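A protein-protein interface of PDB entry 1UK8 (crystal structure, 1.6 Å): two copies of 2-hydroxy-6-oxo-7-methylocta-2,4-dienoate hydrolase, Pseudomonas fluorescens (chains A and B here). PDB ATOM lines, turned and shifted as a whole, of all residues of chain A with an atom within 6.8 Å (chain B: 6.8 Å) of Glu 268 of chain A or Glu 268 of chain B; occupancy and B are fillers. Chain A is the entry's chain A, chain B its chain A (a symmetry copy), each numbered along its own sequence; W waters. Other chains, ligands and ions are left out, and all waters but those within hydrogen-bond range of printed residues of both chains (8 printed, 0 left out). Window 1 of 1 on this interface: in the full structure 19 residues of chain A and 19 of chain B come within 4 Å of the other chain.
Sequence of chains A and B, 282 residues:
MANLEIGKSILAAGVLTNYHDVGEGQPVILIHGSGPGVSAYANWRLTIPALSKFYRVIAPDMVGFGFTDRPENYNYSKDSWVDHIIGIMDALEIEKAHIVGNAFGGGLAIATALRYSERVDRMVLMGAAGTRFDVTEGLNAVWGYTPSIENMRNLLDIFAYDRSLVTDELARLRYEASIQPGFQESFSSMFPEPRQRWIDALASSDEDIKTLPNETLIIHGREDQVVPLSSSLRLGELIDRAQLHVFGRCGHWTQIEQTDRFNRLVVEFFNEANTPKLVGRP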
ATOM      1  N   TYR A  55     -17.694 -10.909  31.776  1.00  0.00           N
ATOM      2  CA  TYR A  55     -17.198 -12.146  31.175  1.00  0.00           C
ATOM      3  C   TYR A  55     -17.140 -13.286  32.172  1.00  0.00           C
ATOM      4  O   TYR A  55     -17.240 -13.074  33.378  1.00  0.00           O
ATOM      5  CB  TYR A  55     -15.778 -11.919  30.639  1.00  0.00           C
ATOM      6  CG  TYR A  55     -15.717 -10.935  29.506  1.00  0.00           C
ATOM      7  CD1 TYR A  55     -15.956 -11.346  28.200  1.00  0.00           C
ATOM      8  CD2 TYR A  55     -15.504  -9.577  29.744  1.00  0.00           C
ATOM      9  CE1 TYR A  55     -15.995 -10.437  27.156  1.00  0.00           C
ATOM     10  CE2 TYR A  55     -15.543  -8.653  28.702  1.00  0.00           C
ATOM     11  CZ  TYR A  55     -15.792  -9.093  27.412  1.00  0.00           C
ATOM     12  OH  TYR A  55     -15.875  -8.196  26.372  1.00  0.00           O
ATOM     13  N   ARG A 122      -9.150 -13.430  21.292  1.00  0.00           N
ATOM     14  CA  ARG A 122      -8.229 -12.316  21.499  1.00  0.00           C
ATOM     15  C   ARG A 122      -7.236 -12.628  22.612  1.00  0.00           C
ATOM     16  O   ARG A 122      -7.514 -13.439  23.499  1.00  0.00           O
ATOM     17  CB  ARG A 122      -8.995 -11.027  21.821  1.00  0.00           C
ATOM     18  CG  ARG A 122      -9.903 -10.574  20.685  1.00  0.00           C
ATOM     19  CD  ARG A 122     -10.314  -9.115  20.813  1.00  0.00           C
ATOM     20  NE  ARG A 122     -10.939  -8.659  19.573  1.00  0.00           N
ATOM     21  CZ  ARG A 122     -11.053  -7.387  19.212  1.00  0.00           C
ATOM     22  NH1 ARG A 122     -10.585  -6.425  20.001  1.00  0.00           N
ATOM     23  NH2 ARG A 122     -11.609  -7.076  18.049  1.00  0.00           N
ATOM     24  N   ARG A 261      -6.509   1.268  35.327  1.00  0.00           N
ATOM     25  CA  ARG A 261      -6.175   1.502  33.923  1.00  0.00           C
ATOM     26  C   ARG A 261      -6.138   0.176  33.168  1.00  0.00           C
ATOM     27  O   ARG A 261      -6.667   0.053  32.061  1.00  0.00           O
ATOM     28  CB  ARG A 261      -4.809   2.179  33.806  1.00  0.00           C
ATOM     29  CG  ARG A 261      -4.779   3.615  34.283  1.00  0.00           C
ATOM     30  CD  ARG A 261      -3.369   4.171  34.219  1.00  0.00           C
ATOM     31  NE  ARG A 261      -3.343   5.611  34.452  1.00  0.00           N
ATOM     32  CZ  ARG A 261      -2.235   6.343  34.467  1.00  0.00           C
ATOM     33  NH1 ARG A 261      -1.054   5.772  34.271  1.00  0.00           N
ATOM     34  NH2 ARG A 261      -2.310   7.654  34.659  1.00  0.00           N
ATOM     35  N   ASN A 263      -7.581  -2.783  33.962  1.00  0.00           N
ATOM     36  CA  ASN A 263      -8.901  -3.382  33.829  1.00  0.00           C
ATOM     37  C   ASN A 263      -9.744  -2.704  32.757  1.00  0.00           C
ATOM     38  O   ASN A 263     -10.416  -3.378  31.977  1.00  0.00           O
ATOM     39  CB  ASN A 263      -9.626  -3.372  35.177  1.00  0.00           C
ATOM     40  CG  ASN A 263      -8.986  -4.311  36.182  1.00  0.00           C
ATOM     41  OD1 ASN A 263      -8.269  -5.242  35.808  1.00  0.00           O
ATOM     42  ND2 ASN A 263      -9.252  -4.084  37.464  1.00  0.00           N
ATOM     43  N   ARG A 264      -9.702  -1.374  32.712  1.00  0.00           N
ATOM     44  CA  ARG A 264     -10.459  -0.628  31.711  1.00  0.00           C
ATOM     45  C   ARG A 264      -9.994  -0.993  30.301  1.00  0.00           C
ATOM     46  O   ARG A 264     -10.812  -1.244  29.413  1.00  0.00           O
ATOM     47  CB  ARG A 264     -10.286   0.878  31.919  1.00  0.00           C
ATOM     48  CG  ARG A 264     -11.286   1.514  32.863  1.00  0.00           C
ATOM     49  CD  ARG A 264     -11.006   3.003  32.991  1.00  0.00           C
ATOM     50  NE  ARG A 264      -9.855   3.266  33.852  1.00  0.00           N
ATOM     51  CZ  ARG A 264      -9.115   4.368  33.799  1.00  0.00           C
ATOM     52  NH1 ARG A 264      -8.091   4.526  34.627  1.00  0.00           N
ATOM     53  NH2 ARG A 264      -9.386   5.306  32.902  1.00  0.00           N
ATOM     54  N   LEU A 265      -8.679  -1.012  30.103  1.00  0.00           N
ATOM     55  CA  LEU A 265      -8.102  -1.346  28.805  1.00  0.00           C
ATOM     56  C   LEU A 265      -8.478  -2.744  28.341  1.00  0.00           C
ATOM     57  O   LEU A 265      -8.886  -2.939  27.195  1.00  0.00           O
ATOM     58  CB  LEU A 265      -6.577  -1.230  28.854  1.00  0.00           C
ATOM     59  CG  LEU A 265      -5.956   0.151  28.659  1.00  0.00           C
ATOM     60  CD1 LEU A 265      -4.465   0.083  28.961  1.00  0.00           C
ATOM     61  CD2 LEU A 265      -6.196   0.620  27.226  1.00  0.00           C
ATOM     62  N   VAL A 266      -8.335  -3.718  29.233  1.00  0.00           N
ATOM     63  CA  VAL A 266      -8.643  -5.101  28.895  1.00  0.00           C
ATOM     64  C   VAL A 266     -10.131  -5.321  28.616  1.00  0.00           C
ATOM     65  O   VAL A 266     -10.488  -5.960  27.626  1.00  0.00           O
ATOM     66  CB  VAL A 266      -8.169  -6.053  30.013  1.00  0.00           C
ATOM     67  CG1 VAL A 266      -8.631  -7.473  29.725  1.00  0.00           C
ATOM     68  CG2 VAL A 266      -6.648  -6.011  30.109  1.00  0.00           C
ATOM     69  N   VAL A 267     -11.000  -4.791  29.471  1.00  0.00           N
ATOM     70  CA  VAL A 267     -12.435  -4.964  29.257  1.00  0.00           C
ATOM     71  C   VAL A 267     -12.888  -4.354  27.930  1.00  0.00           C
ATOM     72  O   VAL A 267     -13.617  -4.993  27.171  1.00  0.00           O
ATOM     73  CB  VAL A 267     -13.269  -4.341  30.406  1.00  0.00           C
ATOM     74  CG1 VAL A 267     -14.753  -4.378  30.047  1.00  0.00           C
ATOM     75  CG2 VAL A 267     -13.034  -5.115  31.695  1.00  0.00           C
ATOM     76  N   GLU A 268     -12.454  -3.127  27.647  1.00  0.00           N
ATOM     77  CA  GLU A 268     -12.839  -2.472  26.399  1.00  0.00           C
ATOM     78  C   GLU A 268     -12.267  -3.209  25.195  1.00  0.00           C
ATOM     79  O   GLU A 268     -12.895  -3.264  24.137  1.00  0.00           O
ATOM     80  CB  GLU A 268     -12.379  -1.012  26.394  1.00  0.00           C
ATOM     81  CG  GLU A 268     -13.059  -0.164  27.457  1.00  0.00           C
ATOM     82  CD  GLU A 268     -12.656   1.296  27.391  1.00  0.00           C
ATOM     83  OE1 GLU A 268     -11.441   1.576  27.377  1.00  0.00           O
ATOM     84  OE2 GLU A 268     -13.556   2.163  27.363  1.00  0.00           O
ATOM     85  N   PHE A 269     -11.078  -3.779  25.363  1.00  0.00           N
ATOM     86  CA  PHE A 269     -10.431  -4.532  24.295  1.00  0.00           C
ATOM     87  C   PHE A 269     -11.279  -5.756  23.951  1.00  0.00           C
ATOM     88  O   PHE A 269     -11.519  -6.040  22.780  1.00  0.00           O
ATOM     89  CB  PHE A 269      -9.023  -4.961  24.734  1.00  0.00           C
ATOM     90  CG  PHE A 269      -8.317  -5.869  23.756  1.00  0.00           C
ATOM     91  CD1 PHE A 269      -8.019  -5.441  22.463  1.00  0.00           C
ATOM     92  CD2 PHE A 269      -7.924  -7.147  24.143  1.00  0.00           C
ATOM     93  CE1 PHE A 269      -7.336  -6.274  21.571  1.00  0.00           C
ATOM     94  CE2 PHE A 269      -7.244  -7.988  23.263  1.00  0.00           C
ATOM     95  CZ  PHE A 269      -6.948  -7.552  21.973  1.00  0.00           C
ATOM     96  N   PHE A 270     -11.737  -6.478  24.972  1.00  0.00           N
ATOM     97  CA  PHE A 270     -12.561  -7.658  24.731  1.00  0.00           C
ATOM     98  C   PHE A 270     -13.957  -7.260  24.257  1.00  0.00           C
ATOM     99  O   PHE A 270     -14.558  -7.956  23.440  1.00  0.00           O
ATOM    100  CB  PHE A 270     -12.667  -8.528  25.995  1.00  0.00           C
ATOM    101  CG  PHE A 270     -11.375  -9.204  26.387  1.00  0.00           C
ATOM    102  CD1 PHE A 270     -10.431  -9.555  25.426  1.00  0.00           C
ATOM    103  CD2 PHE A 270     -11.118  -9.515  27.721  1.00  0.00           C
ATOM    104  CE1 PHE A 270      -9.249 -10.208  25.786  1.00  0.00           C
ATOM    105  CE2 PHE A 270      -9.940 -10.169  28.091  1.00  0.00           C
ATOM    106  CZ  PHE A 270      -9.003 -10.515  27.121  1.00  0.00           C
ATOM    107  N   ASN A 271     -14.470  -6.140  24.763  1.00  0.00           N
ATOM    108  CA  ASN A 271     -15.797  -5.667  24.366  1.00  0.00           C
ATOM    109  C   ASN A 271     -15.860  -5.443  22.857  1.00  0.00           C
ATOM    110  O   ASN A 271     -16.918  -5.592  22.242  1.00  0.00           O
ATOM    111  CB  ASN A 271     -16.145  -4.353  25.081  1.00  0.00           C
ATOM    112  CG  ASN A 271     -16.566  -4.552  26.529  1.00  0.00           C
ATOM    113  OD1 ASN A 271     -16.816  -3.581  27.246  1.00  0.00           O
ATOM    114  ND2 ASN A 271     -16.654  -5.801  26.964  1.00  0.00           N
ATOM    115  N   GLU A 272     -14.723  -5.082  22.269  1.00  0.00           N
ATOM    116  CA  GLU A 272     -14.632  -4.819  20.837  1.00  0.00           C
ATOM    117  C   GLU A 272     -15.007  -6.048  20.011  1.00  0.00           C
ATOM    118  O   GLU A 272     -15.560  -5.926  18.918  1.00  0.00           O
ATOM    119  CB  GLU A 272     -13.211  -4.379  20.476  1.00  0.00           C
ATOM    120  CG  GLU A 272     -13.143  -3.123  19.631  1.00  0.00           C
ATOM    121  CD  GLU A 272     -11.740  -2.832  19.129  1.00  0.00           C
ATOM    122  OE1 GLU A 272     -11.530  -1.741  18.560  1.00  0.00           O
ATOM    123  OE2 GLU A 272     -10.851  -3.695  19.294  1.00  0.00           O
ATOM    124  N   ALA A 273     -14.697  -7.229  20.538  1.00  0.00           N
ATOM    125  CA  ALA A 273     -15.004  -8.479  19.852  1.00  0.00           C
ATOM    126  C   ALA A 273     -16.514  -8.691  19.763  1.00  0.00           C
ATOM    127  O   ALA A 273     -17.006  -8.932  18.641  1.00  0.00           O
ATOM    128  CB  ALA A 273     -14.353  -9.650  20.582  1.00  0.00           C
ATOM    129  N   TYR B  55     -16.788  16.986  27.596  1.00  0.00           N
ATOM    130  CA  TYR B  55     -15.872  18.112  27.767  1.00  0.00           C
ATOM    131  C   TYR B  55     -16.216  19.275  26.857  1.00  0.00           C
ATOM    132  O   TYR B  55     -16.997  19.132  25.920  1.00  0.00           O
ATOM    133  CB  TYR B  55     -14.443  17.663  27.433  1.00  0.00           C
ATOM    134  CG  TYR B  55     -13.904  16.632  28.384  1.00  0.00           C
ATOM    135  CD1 TYR B  55     -13.316  17.016  29.583  1.00  0.00           C
ATOM    136  CD2 TYR B  55     -14.054  15.269  28.126  1.00  0.00           C
ATOM    137  CE1 TYR B  55     -12.898  16.077  30.511  1.00  0.00           C
ATOM    138  CE2 TYR B  55     -13.639  14.316  29.053  1.00  0.00           C
ATOM    139  CZ  TYR B  55     -13.065  14.730  30.244  1.00  0.00           C
ATOM    140  OH  TYR B  55     -12.683  13.810  31.193  1.00  0.00           O
ATOM    141  N   ARG B 122      -3.608  17.809  31.452  1.00  0.00           N
ATOM    142  CA  ARG B 122      -3.126  16.584  30.817  1.00  0.00           C
ATOM    143  C   ARG B 122      -2.886  16.801  29.327  1.00  0.00           C
ATOM    144  O   ARG B 122      -3.491  17.680  28.710  1.00  0.00           O
ATOM    145  CB  ARG B 122      -4.116  15.433  31.031  1.00  0.00           C
ATOM    146  CG  ARG B 122      -4.293  15.065  32.498  1.00  0.00           C
ATOM    147  CD  ARG B 122      -4.910  13.686  32.684  1.00  0.00           C
ATOM    148  NE  ARG B 122      -4.798  13.270  34.080  1.00  0.00           N
ATOM    149  CZ  ARG B 122      -4.872  12.013  34.498  1.00  0.00           C
ATOM    150  NH1 ARG B 122      -5.063  11.029  33.625  1.00  0.00           N
ATOM    151  NH2 ARG B 122      -4.726  11.734  35.787  1.00  0.00           N
ATOM    152  N   ARG B 261     -11.325   3.507  18.966  1.00  0.00           N
ATOM    153  CA  ARG B 261     -10.306   3.168  19.957  1.00  0.00           C
ATOM    154  C   ARG B 261      -9.668   4.440  20.506  1.00  0.00           C
ATOM    155  O   ARG B 261      -9.469   4.590  21.713  1.00  0.00           O
ATOM    156  CB  ARG B 261      -9.218   2.299  19.325  1.00  0.00           C
ATOM    157  CG  ARG B 261      -9.663   0.895  18.975  1.00  0.00           C
ATOM    158  CD  ARG B 261      -8.551   0.142  18.269  1.00  0.00           C
ATOM    159  NE  ARG B 261      -8.863  -1.276  18.124  1.00  0.00           N
ATOM    160  CZ  ARG B 261      -8.068  -2.157  17.528  1.00  0.00           C
ATOM    161  NH1 ARG B 261      -6.910  -1.769  17.010  1.00  0.00           N
ATOM    162  NH2 ARG B 261      -8.422  -3.435  17.467  1.00  0.00           N
ATOM    163  N   ASN B 263     -10.870   7.606  20.520  1.00  0.00           N
ATOM    164  CA  ASN B 263     -11.792   8.381  21.337  1.00  0.00           C
ATOM    165  C   ASN B 263     -11.985   7.783  22.724  1.00  0.00           C
ATOM    166  O   ASN B 263     -12.007   8.512  23.717  1.00  0.00           O
ATOM    167  CB  ASN B 263     -13.137   8.532  20.620  1.00  0.00           C
ATOM    168  CG  ASN B 263     -13.037   9.414  19.389  1.00  0.00           C
ATOM    169  OD1 ASN B 263     -12.109  10.216  19.262  1.00  0.00           O
ATOM    170  ND2 ASN B 263     -13.999   9.283  18.482  1.00  0.00           N
ATOM    171  N   ARG B 264     -12.115   6.461  22.796  1.00  0.00           N
ATOM    172  CA  ARG B 264     -12.285   5.787  24.081  1.00  0.00           C
ATOM    173  C   ARG B 264     -11.070   6.021  24.977  1.00  0.00           C
ATOM    174  O   ARG B 264     -11.211   6.347  26.158  1.00  0.00           O
ATOM    175  CB  ARG B 264     -12.473   4.283  23.877  1.00  0.00           C
ATOM    176  CG  ARG B 264     -13.908   3.836  23.675  1.00  0.00           C
ATOM    177  CD  ARG B 264     -13.961   2.329  23.478  1.00  0.00           C
ATOM    178  NE  ARG B 264     -13.534   1.943  22.135  1.00  0.00           N
ATOM    179  CZ  ARG B 264     -13.054   0.746  21.817  1.00  0.00           C
ATOM    180  NH1 ARG B 264     -12.697   0.480  20.568  1.00  0.00           N
ATOM    181  NH2 ARG B 264     -12.912  -0.182  22.753  1.00  0.00           N
ATOM    182  N   LEU B 265      -9.880   5.844  24.411  1.00  0.00           N
ATOM    183  CA  LEU B 265      -8.639   6.036  25.154  1.00  0.00           C
ATOM    184  C   LEU B 265      -8.490   7.452  25.688  1.00  0.00           C
ATOM    185  O   LEU B 265      -8.160   7.652  26.857  1.00  0.00           O
ATOM    186  CB  LEU B 265      -7.433   5.706  24.271  1.00  0.00           C
ATOM    187  CG  LEU B 265      -7.012   4.243  24.149  1.00  0.00           C
ATOM    188  CD1 LEU B 265      -5.948   4.112  23.067  1.00  0.00           C
ATOM    189  CD2 LEU B 265      -6.480   3.752  25.493  1.00  0.00           C
ATOM    190  N   VAL B 266      -8.730   8.433  24.826  1.00  0.00           N
ATOM    191  CA  VAL B 266      -8.598   9.830  25.217  1.00  0.00           C
ATOM    192  C   VAL B 266      -9.631  10.247  26.265  1.00  0.00           C
ATOM    193  O   VAL B 266      -9.284  10.886  27.258  1.00  0.00           O
ATOM    194  CB  VAL B 266      -8.694  10.752  23.984  1.00  0.00           C
ATOM    195  CG1 VAL B 266      -8.711  12.209  24.417  1.00  0.00           C
ATOM    196  CG2 VAL B 266      -7.508  10.499  23.061  1.00  0.00           C
ATOM    197  N   VAL B 267     -10.893   9.883  26.060  1.00  0.00           N
ATOM    198  CA  VAL B 267     -11.926  10.249  27.027  1.00  0.00           C
ATOM    199  C   VAL B 267     -11.647   9.653  28.407  1.00  0.00           C
ATOM    200  O   VAL B 267     -11.732  10.356  29.415  1.00  0.00           O
ATOM    201  CB  VAL B 267     -13.336   9.802  26.563  1.00  0.00           C
ATOM    202  CG1 VAL B 267     -14.347  10.034  27.684  1.00  0.00           C
ATOM    203  CG2 VAL B 267     -13.749  10.590  25.328  1.00  0.00           C
ATOM    204  N   GLU B 268     -11.309   8.366  28.455  1.00  0.00           N
ATOM    205  CA  GLU B 268     -11.025   7.719  29.734  1.00  0.00           C
ATOM    206  C   GLU B 268      -9.783   8.314  30.384  1.00  0.00           C
ATOM    207  O   GLU B 268      -9.702   8.411  31.610  1.00  0.00           O
ATOM    208  CB  GLU B 268     -10.853   6.209  29.546  1.00  0.00           C
ATOM    209  CG  GLU B 268     -12.121   5.513  29.078  1.00  0.00           C
ATOM    210  CD  GLU B 268     -11.961   4.010  28.971  1.00  0.00           C
ATOM    211  OE1 GLU B 268     -10.998   3.559  28.321  1.00  0.00           O
ATOM    212  OE2 GLU B 268     -12.807   3.279  29.532  1.00  0.00           O
ATOM    213  N   PHE B 269      -8.820   8.716  29.559  1.00  0.00           N
ATOM    214  CA  PHE B 269      -7.590   9.322  30.055  1.00  0.00           C
ATOM    215  C   PHE B 269      -7.920  10.638  30.758  1.00  0.00           C
ATOM    216  O   PHE B 269      -7.426  10.903  31.852  1.00  0.00           O
ATOM    217  CB  PHE B 269      -6.619   9.564  28.890  1.00  0.00           C
ATOM    218  CG  PHE B 269      -5.368  10.320  29.271  1.00  0.00           C
ATOM    219  CD1 PHE B 269      -4.467   9.798  30.199  1.00  0.00           C
ATOM    220  CD2 PHE B 269      -5.080  11.545  28.676  1.00  0.00           C
ATOM    221  CE1 PHE B 269      -3.294  10.486  30.524  1.00  0.00           C
ATOM    222  CE2 PHE B 269      -3.913  12.241  28.993  1.00  0.00           C
ATOM    223  CZ  PHE B 269      -3.017  11.712  29.919  1.00  0.00           C
ATOM    224  N   PHE B 270      -8.760  11.462  30.134  1.00  0.00           N
ATOM    225  CA  PHE B 270      -9.133  12.735  30.740  1.00  0.00           C
ATOM    226  C   PHE B 270     -10.071  12.519  31.925  1.00  0.00           C
ATOM    227  O   PHE B 270     -10.010  13.258  32.907  1.00  0.00           O
ATOM    228  CB  PHE B 270      -9.798  13.665  29.711  1.00  0.00           C
ATOM    229  CG  PHE B 270      -8.861  14.167  28.638  1.00  0.00           C
ATOM    230  CD1 PHE B 270      -7.504  14.338  28.897  1.00  0.00           C
ATOM    231  CD2 PHE B 270      -9.346  14.496  27.375  1.00  0.00           C
ATOM    232  CE1 PHE B 270      -6.641  14.831  27.914  1.00  0.00           C
ATOM    233  CE2 PHE B 270      -8.493  14.991  26.385  1.00  0.00           C
ATOM    234  CZ  PHE B 270      -7.138  15.157  26.655  1.00  0.00           C
ATOM    235  N   ASN B 271     -10.931  11.507  31.839  1.00  0.00           N
ATOM    236  CA  ASN B 271     -11.865  11.211  32.926  1.00  0.00           C
ATOM    237  C   ASN B 271     -11.111  10.932  34.224  1.00  0.00           C
ATOM    238  O   ASN B 271     -11.616  11.204  35.316  1.00  0.00           O
ATOM    239  CB  ASN B 271     -12.734   9.992  32.582  1.00  0.00           C
ATOM    240  CG  ASN B 271     -13.856  10.311  31.605  1.00  0.00           C
ATOM    241  OD1 ASN B 271     -14.596   9.418  31.190  1.00  0.00           O
ATOM    242  ND2 ASN B 271     -13.991  11.578  31.237  1.00  0.00           N
ATOM    243  N   GLU B 272      -9.904  10.388  34.097  1.00  0.00           N
ATOM    244  CA  GLU B 272      -9.072  10.054  35.247  1.00  0.00           C
ATOM    245  C   GLU B 272      -8.746  11.286  36.088  1.00  0.00           C
ATOM    246  O   GLU B 272      -8.609  11.196  37.308  1.00  0.00           O
ATOM    247  CB  GLU B 272      -7.770   9.400  34.777  1.00  0.00           C
ATOM    248  CG  GLU B 272      -7.424   8.112  35.496  1.00  0.00           C
ATOM    249  CD  GLU B 272      -6.037   7.602  35.146  1.00  0.00           C
ATOM    250  OE1 GLU B 272      -5.705   6.469  35.550  1.00  0.00           O
ATOM    251  OE2 GLU B 272      -5.277   8.336  34.479  1.00  0.00           O
ATOM    252  N   ALA B 273      -8.617  12.433  35.427  1.00  0.00           N
ATOM    253  CA  ALA B 273      -8.310  13.683  36.113  1.00  0.00           C
ATOM    254  C   ALA B 273      -9.467  14.104  37.016  1.00  0.00           C
ATOM    255  O   ALA B 273      -9.214  14.363  38.210  1.00  0.00           O
ATOM    256  CB  ALA B 273      -8.015  14.779  35.095  1.00  0.00           C
HETATM  257  O   HOH W   1      -9.008  -2.393  21.356  1.00  0.00           O
HETATM  258  O   HOH W   2      -4.570   5.257  37.646  1.00  0.00           O
HETATM  259  O   HOH W   3     -13.012   0.414  30.380  1.00  0.00           O
HETATM  260  O   HOH W   4     -11.255   6.768  33.341  1.00  0.00           O
HETATM  261  O   HOH W   5      -5.097   6.877  31.799  1.00  0.00           O
HETATM  262  O   HOH W   6     -14.896  -1.343  23.489  1.00  0.00           O
HETATM  263  O   HOH W   7     -11.591  -0.613  16.137  1.00  0.00           O
HETATM  264  O   HOH W   8     -13.787   5.062  26.648  1.00  0.00           O
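The backbone carbonyl oxygen (O) of Glu 268 of chain A is in hydrogen-bond range of the guanidinium group (NH2) of Arg 264 of chain B.
The side-chain carboxylate (OE1) of Glu 272 of chain A lies within salt-bridge range of the guanidinium group (NE) of Arg 261 of chain B.
OE1 of Glu 272 of chain A lies within salt-bridge range of NH1 of Arg 264 of chain B (3.2 Å).
The guanidinium group of Arg 261 of chain A lies within salt-bridge range of the side-chain carboxylate of Glu 272 of chain B.
NH1 of Arg 264 of chain A lies within salt-bridge range of OE1 of Glu 272 of chain B, at 3.2 Å.
The backbone carbonyl oxygen (O) of Glu 268 of chain B lies within hydrogen-bond range of the guanidinium group (NH2) of Arg 264 of chain A (3.4 Å).
OE2 of Glu 268 of chain A sits close to OE2 of Glu 268 of chain B, 2.6 Å away.
Arg 261 of chain A touches Glu 272 of chain B, and with the chains exchanged Glu 272 of chain A touches Arg 261 of chain B.
Arg 264 of chain A touches Glu 268 of chain B, and with the chains exchanged Glu 268 of chain A touches Arg 264 of chain B.
Arg 264 of chain A touches Glu 272 of chain B, and with the chains exchanged Glu 272 of chain A touches Arg 264 of chain B.
Glu 268 of chain A touches its own counterpart, Glu 268 of chain B.
Hydrophobic or aromatic side chains of chain B within 4 Å of the printed part of chain A: Leu 265.
Printed residues of chain A that touch a printed residue of chain B: Arg 261, Arg 264, Leu 265, Glu 268 and Glu 272.
Hydrophobic or aromatic side chains of chain A within 4 Å of the printed part of chain B: Leu 265.
Among the printed residues, 8 pairs touch across the chains.
Among the printed residues, Asp or Glu carboxylates within 4 Å of a Lys or Arg side-chain nitrogen of the other chain: Arg 261 of chain A with Glu 272 of chain B, Arg 264 of chain A with Glu 272 of chain B, Glu 272 of chain A with Arg 261 of chain B and Glu 272 of chain A with Arg 264 of chain B.
The guanidinium group (NH1) of Arg 122 of chain A is in salt-bridge range of the side-chain carboxylate (OE2) of Glu 272 of chain A.
The side-chain carboxylate (OE2) of Glu 272 of chain B lies within salt-bridge range of the guanidinium group (NH1) of Arg 122 of chain B.
CD2 of Leu 265 of chain B touches CD2 of Leu 265 of chain A, 3.6 Å away.
Water W4 lies within hydrogen-bond range of NH2 of Arg 264 of chain A and O of Glu 268 of chain B.
Water W6 lies within hydrogen-bond range of the guanidinium group of Arg 264 of chain B and the backbone carbonyl oxygen of Glu 268 of chain A.
Water W7 lies within hydrogen-bond range of the side-chain carboxylate of Glu 272 of chain A and the guanidinium group of Arg 261 of chain B.
Water W8 bridges the backbone carbonyl oxygen (O) of Arg 264 of chain B (2.9 Å) and the side-chain carboxylate (OE2) of Glu 268 of chain A (3.0 Å).
Water W1 bridges the side-chain carboxylate (OE2) of Glu 272 of chain A (3.1 Å) and the guanidinium group (NE) of Arg 261 of chain B (3.4 Å).
Water W5 lies within hydrogen-bond range of the side-chain carboxylate of Glu 272 of chain B and the guanidinium group of Arg 261 of chain A.
Glu 268 of chain A touches two residues of chain B.
Of chain A, only Arg 264 and Glu 268 come within 4 Å of Glu 268 of chain B.
Of the printed residues of chain B, Arg 261 of chain A touches Glu 272.
Printed residues of chain A within 4 Å of Arg 264 of chain B: Glu 268 and Glu 272.
Of the printed residues of chain A, Glu 272 of chain B touches Arg 261 (2.7 Å) and Arg 264 (3.2 Å).
Asn 263 of chain A touches none of the printed residues of chain B.
The nearest residue of chain A that does not touch Glu 268 of chain B is Leu 265 of chain A (5.4 Å).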
